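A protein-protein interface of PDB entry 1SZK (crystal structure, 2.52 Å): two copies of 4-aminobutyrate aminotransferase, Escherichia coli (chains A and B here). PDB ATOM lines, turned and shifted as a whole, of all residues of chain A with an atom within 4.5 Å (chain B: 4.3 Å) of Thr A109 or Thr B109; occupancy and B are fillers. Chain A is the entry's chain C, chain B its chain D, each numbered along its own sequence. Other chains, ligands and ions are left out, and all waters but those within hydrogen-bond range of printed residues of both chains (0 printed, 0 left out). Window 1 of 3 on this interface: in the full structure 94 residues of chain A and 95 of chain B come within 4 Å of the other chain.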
ATOM      1  N   VAL A 108      20.257 -24.167  19.223  1.00  0.00           N
ATOM      2  CA  VAL A 108      20.380 -22.880  19.891  1.00  0.00           C
ATOM      3  C   VAL A 108      21.775 -22.885  20.510  1.00  0.00           C
ATOM      4  O   VAL A 108      22.662 -23.568  19.987  1.00  0.00           O
ATOM      5  CB  VAL A 108      19.283 -22.705  20.972  1.00  0.00           C
ATOM      6  CG1 VAL A 108      17.904 -22.760  20.313  1.00  0.00           C
ATOM      7  CG2 VAL A 108      19.402 -23.790  22.027  1.00  0.00           C
ATOM      8  N   THR A 109      21.986 -22.146  21.602  1.00  0.00           N
ATOM      9  CA  THR A 109      23.300 -22.121  22.237  1.00  0.00           C
ATOM     10  C   THR A 109      23.353 -22.673  23.652  1.00  0.00           C
ATOM     11  O   THR A 109      24.317 -23.359  24.005  1.00  0.00           O
ATOM     12  CB  THR A 109      23.890 -20.706  22.269  1.00  0.00           C
ATOM     13  OG1 THR A 109      23.848 -20.132  20.951  1.00  0.00           O
ATOM     14  CG2 THR A 109      25.346 -20.760  22.756  1.00  0.00           C
ATOM     15  N   THR A 110      22.331 -22.389  24.469  1.00  0.00           N
ATOM     16  CA  THR A 110      22.324 -22.866  25.866  1.00  0.00           C
ATOM     17  C   THR A 110      21.090 -23.670  26.271  1.00  0.00           C
ATOM     18  O   THR A 110      20.023 -23.558  25.654  1.00  0.00           O
ATOM     19  CB  THR A 110      22.469 -21.691  26.898  1.00  0.00           C
ATOM     20  OG1 THR A 110      21.313 -20.851  26.842  1.00  0.00           O
ATOM     21  CG2 THR A 110      23.706 -20.846  26.606  1.00  0.00           C
ATOM     22  N   GLU A 113      18.123 -21.636  26.616  1.00  0.00           N
ATOM     23  CA  GLU A 113      17.520 -21.293  25.338  1.00  0.00           C
ATOM     24  C   GLU A 113      16.729 -22.481  24.815  1.00  0.00           C
ATOM     25  O   GLU A 113      15.635 -22.327  24.279  1.00  0.00           O
ATOM     26  CB  GLU A 113      18.595 -20.890  24.327  1.00  0.00           C
ATOM     27  CG  GLU A 113      19.394 -19.689  24.758  1.00  0.00           C
ATOM     28  CD  GLU A 113      20.248 -19.113  23.647  1.00  0.00           C
ATOM     29  OE1 GLU A 113      20.933 -19.887  22.940  1.00  0.00           O
ATOM     30  OE2 GLU A 113      20.249 -17.876  23.492  1.00  0.00           O
ATOM     31  N   PRO A 275      30.122 -24.360  23.671  1.00  0.00           N
ATOM     32  CA  PRO A 275      28.776 -23.755  23.674  1.00  0.00           C
ATOM     33  C   PRO A 275      27.757 -24.195  22.615  1.00  0.00           C
ATOM     34  O   PRO A 275      27.719 -23.640  21.513  1.00  0.00           O
ATOM     35  CB  PRO A 275      29.060 -22.250  23.584  1.00  0.00           C
ATOM     36  CG  PRO A 275      30.476 -22.114  24.103  1.00  0.00           C
ATOM     37  CD  PRO A 275      31.165 -23.329  23.535  1.00  0.00           C
ATOM     38  N   LEU A 276      26.904 -25.155  22.966  1.00  0.00           N
ATOM     39  CA  LEU A 276      25.882 -25.624  22.040  1.00  0.00           C
ATOM     40  C   LEU A 276      24.702 -26.292  22.738  1.00  0.00           C
ATOM     41  O   LEU A 276      24.863 -26.946  23.761  1.00  0.00           O
ATOM     42  CB  LEU A 276      26.490 -26.609  21.034  1.00  0.00           C
ATOM     43  CG  LEU A 276      25.460 -27.217  20.078  1.00  0.00           C
ATOM     44  CD1 LEU A 276      25.363 -26.368  18.829  1.00  0.00           C
ATOM     45  CD2 LEU A 276      25.844 -28.625  19.733  1.00  0.00           C
ATOM     46  N   ALA A 277      23.515 -26.132  22.162  1.00  0.00           N
ATOM     47  CA  ALA A 277      22.296 -26.734  22.686  1.00  0.00           C
ATOM     48  C   ALA A 277      21.255 -26.825  21.560  1.00  0.00           C
ATOM     49  O   ALA A 277      21.425 -26.218  20.493  1.00  0.00           O
ATOM     50  CB  ALA A 277      21.747 -25.899  23.842  1.00  0.00           C
ATOM     51  N   TYR A 298      24.264 -16.704  17.929  1.00  0.00           N
ATOM     52  CA  TYR A 298      25.320 -17.729  17.980  1.00  0.00           C
ATOM     53  C   TYR A 298      24.807 -19.149  17.795  1.00  0.00           C
ATOM     54  O   TYR A 298      25.586 -20.107  17.830  1.00  0.00           O
ATOM     55  CB  TYR A 298      26.037 -17.706  19.333  1.00  0.00           C
ATOM     56  CG  TYR A 298      26.750 -16.435  19.695  1.00  0.00           C
ATOM     57  CD1 TYR A 298      27.630 -15.821  18.804  1.00  0.00           C
ATOM     58  CD2 TYR A 298      26.639 -15.908  20.987  1.00  0.00           C
ATOM     59  CE1 TYR A 298      28.392 -14.719  19.197  1.00  0.00           C
ATOM     60  CE2 TYR A 298      27.394 -14.811  21.387  1.00  0.00           C
ATOM     61  CZ  TYR A 298      28.273 -14.224  20.493  1.00  0.00           C
ATOM     62  OH  TYR A 298      29.048 -13.164  20.908  1.00  0.00           O
ATOM     63  N   ALA A 299      23.498 -19.271  17.643  1.00  0.00           N
ATOM     64  CA  ALA A 299      22.827 -20.547  17.492  1.00  0.00           C
ATOM     65  C   ALA A 299      23.565 -21.568  16.628  1.00  0.00           C
ATOM     66  O   ALA A 299      23.955 -21.288  15.500  1.00  0.00           O
ATOM     67  CB  ALA A 299      21.424 -20.306  16.954  1.00  0.00           C
ATOM     68  N   VAL B 108      27.949 -14.233  30.512  1.00  0.00           N
ATOM     69  CA  VAL B 108      26.989 -15.276  30.196  1.00  0.00           C
ATOM     70  C   VAL B 108      27.343 -15.814  28.807  1.00  0.00           C
ATOM     71  O   VAL B 108      28.517 -16.015  28.507  1.00  0.00           O
ATOM     72  CB  VAL B 108      25.547 -14.729  30.260  1.00  0.00           C
ATOM     73  CG1 VAL B 108      25.258 -14.289  31.683  1.00  0.00           C
ATOM     74  CG2 VAL B 108      25.365 -13.552  29.310  1.00  0.00           C
ATOM     75  N   THR B 109      26.369 -16.056  27.944  1.00  0.00           N
ATOM     76  CA  THR B 109      26.748 -16.577  26.644  1.00  0.00           C
ATOM     77  C   THR B 109      26.065 -15.911  25.459  1.00  0.00           C
ATOM     78  O   THR B 109      26.709 -15.641  24.445  1.00  0.00           O
ATOM     79  CB  THR B 109      26.498 -18.077  26.585  1.00  0.00           C
ATOM     80  OG1 THR B 109      26.970 -18.679  27.797  1.00  0.00           O
ATOM     81  CG2 THR B 109      27.242 -18.688  25.405  1.00  0.00           C
ATOM     82  N   THR B 110      24.775 -15.628  25.579  1.00  0.00           N
ATOM     83  CA  THR B 110      24.069 -15.022  24.461  1.00  0.00           C
ATOM     84  C   THR B 110      23.519 -13.669  24.811  1.00  0.00           C
ATOM     85  O   THR B 110      23.240 -13.379  25.978  1.00  0.00           O
ATOM     86  CB  THR B 110      22.884 -15.910  23.967  1.00  0.00           C
ATOM     87  OG1 THR B 110      21.844 -15.922  24.954  1.00  0.00           O
ATOM     88  CG2 THR B 110      23.352 -17.346  23.710  1.00  0.00           C
ATOM     89  N   GLU B 113      20.560 -13.844  27.001  1.00  0.00           N
ATOM     90  CA  GLU B 113      20.856 -14.086  28.399  1.00  0.00           C
ATOM     91  C   GLU B 113      21.387 -12.806  29.040  1.00  0.00           C
ATOM     92  O   GLU B 113      21.109 -12.537  30.199  1.00  0.00           O
ATOM     93  CB  GLU B 113      21.917 -15.156  28.529  1.00  0.00           C
ATOM     94  CG  GLU B 113      21.424 -16.554  28.347  1.00  0.00           C
ATOM     95  CD  GLU B 113      22.539 -17.535  28.556  1.00  0.00           C
ATOM     96  OE1 GLU B 113      23.711 -17.181  28.257  1.00  0.00           O
ATOM     97  OE2 GLU B 113      22.241 -18.654  29.009  1.00  0.00           O
ATOM     98  N   PRO B 275      30.939 -17.510  20.908  1.00  0.00           N
ATOM     99  CA  PRO B 275      29.811 -17.328  21.837  1.00  0.00           C
ATOM    100  C   PRO B 275      30.152 -16.775  23.218  1.00  0.00           C
ATOM    101  O   PRO B 275      30.608 -17.501  24.109  1.00  0.00           O
ATOM    102  CB  PRO B 275      29.185 -18.725  21.920  1.00  0.00           C
ATOM    103  CG  PRO B 275      29.810 -19.495  20.740  1.00  0.00           C
ATOM    104  CD  PRO B 275      31.195 -18.941  20.679  1.00  0.00           C
ATOM    105  N   LEU B 276      29.905 -15.482  23.391  1.00  0.00           N
ATOM    106  CA  LEU B 276      30.173 -14.821  24.651  1.00  0.00           C
ATOM    107  C   LEU B 276      29.261 -13.625  24.775  1.00  0.00           C
ATOM    108  O   LEU B 276      28.981 -12.955  23.793  1.00  0.00           O
ATOM    109  CB  LEU B 276      31.613 -14.329  24.700  1.00  0.00           C
ATOM    110  CG  LEU B 276      31.967 -13.720  26.061  1.00  0.00           C
ATOM    111  CD1 LEU B 276      32.143 -14.843  27.089  1.00  0.00           C
ATOM    112  CD2 LEU B 276      33.216 -12.912  25.942  1.00  0.00           C
ATOM    113  N   ALA B 277      28.806 -13.352  25.985  1.00  0.00           N
ATOM    114  CA  ALA B 277      27.939 -12.206  26.223  1.00  0.00           C
ATOM    115  C   ALA B 277      28.187 -11.802  27.665  1.00  0.00           C
ATOM    116  O   ALA B 277      28.820 -12.547  28.413  1.00  0.00           O
ATOM    117  CB  ALA B 277      26.464 -12.589  26.021  1.00  0.00           C
ATOM    118  N   TYR B 298      27.580 -22.784  30.268  1.00  0.00           N
ATOM    119  CA  TYR B 298      28.609 -22.311  29.359  1.00  0.00           C
ATOM    120  C   TYR B 298      29.149 -20.907  29.671  1.00  0.00           C
ATOM    121  O   TYR B 298      30.244 -20.539  29.236  1.00  0.00           O
ATOM    122  CB  TYR B 298      28.076 -22.356  27.915  1.00  0.00           C
ATOM    123  CG  TYR B 298      27.603 -23.724  27.432  1.00  0.00           C
ATOM    124  CD1 TYR B 298      28.327 -24.885  27.723  1.00  0.00           C
ATOM    125  CD2 TYR B 298      26.468 -23.846  26.619  1.00  0.00           C
ATOM    126  CE1 TYR B 298      27.936 -26.141  27.211  1.00  0.00           C
ATOM    127  CE2 TYR B 298      26.071 -25.089  26.099  1.00  0.00           C
ATOM    128  CZ  TYR B 298      26.809 -26.234  26.397  1.00  0.00           C
ATOM    129  OH  TYR B 298      26.436 -27.461  25.873  1.00  0.00           O
ATOM    130  N   ALA B 299      28.378 -20.136  30.429  1.00  0.00           N
ATOM    131  CA  ALA B 299      28.724 -18.763  30.807  1.00  0.00           C
ATOM    132  C   ALA B 299      30.216 -18.457  30.836  1.00  0.00           C
ATOM    133  O   ALA B 299      30.991 -19.160  31.472  1.00  0.00           O
ATOM    134  CB  ALA B 299      28.098 -18.436  32.159  1.00  0.00           C
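N of Thr A109 lies within hydrogen-bond range of OE1 of Glu A113.
N of Ala A277 is in hydrogen-bond range of O of Thr A109, 3.4 Å away.
OE1 of Glu B113 sits at hydrogen-bond distance from N of Thr B109, at 2.9 Å.
The backbone carbonyl oxygen of Thr B109 lies close to the backbone NH of Ala B277.
The side-chain hydroxyl (OG1) of Thr B109 lies within hydrogen-bond range of the backbone NH (N) of Ala B299 (3.3 Å).
N of Glu B113 is in hydrogen-bond range of OG1 of Thr B110 (3.2 Å).
Thr B109 touches its own counterpart, Thr A109.
Thr A109 touches Thr B110, and with the chains exchanged Thr A110 touches Thr B109.
Pro A275 touches its own counterpart, Pro B275.
Pro A275 touches Tyr B298, and with the chains exchanged Tyr A298 touches Pro B275.
9 positions are printed for both chains.
The side-chain hydroxyl (OG1) of Thr A110 sits at hydrogen-bond distance from the side-chain carboxylate (OE2) of Glu B113 (3.2 Å).
OE2 of Glu A113 sits at hydrogen-bond distance from OG1 of Thr B110 (2.9 Å).
The backbone carbonyl oxygen (O) of Leu A276 lies within hydrogen-bond range of the side-chain hydroxyl (OH) of Tyr B298 (2.7 Å).
The side-chain hydroxyl of Tyr A298 sits at hydrogen-bond distance from the backbone carbonyl oxygen of Leu B276 (2.9 Å).
Along chain A the printed residues that touch a printed residue of chain B span positions 109 to 298.
Of the 9 printed residues of chain B, 6 touch a printed residue of chain A.
Among the printed residues, no Asp or Glu carboxylate lies within 4 Å of a Lys or Arg side-chain nitrogen of the other chain.
Among the printed residues, merely in contact across the chains: Thr A109 with Tyr B298, Tyr A298 with Thr B109, Tyr A298 with Pro B275, Thr A109 with Thr B110, Pro A275 with Tyr B298, Thr A109 with Thr B109, Pro A275 with Pro B275 and Thr A110 with Thr B109.
Val A108 touches none of the printed residues of chain B.
Thr A109 touches three residues of chain B.
Of the printed residues of chain B, Glu A113 touches Thr B110 (2.9 Å).
Printed residues of chain B within 4 Å of Pro A275: Pro B275 (3.9 Å) and Tyr B298 (3.7 Å).
Val B108 touches none of the printed residues of chain A.
Thr B109 touches three residues of chain A.
The nearest printed residue of chain A that does not touch Leu B276 is Pro A275 (6.7 Å).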
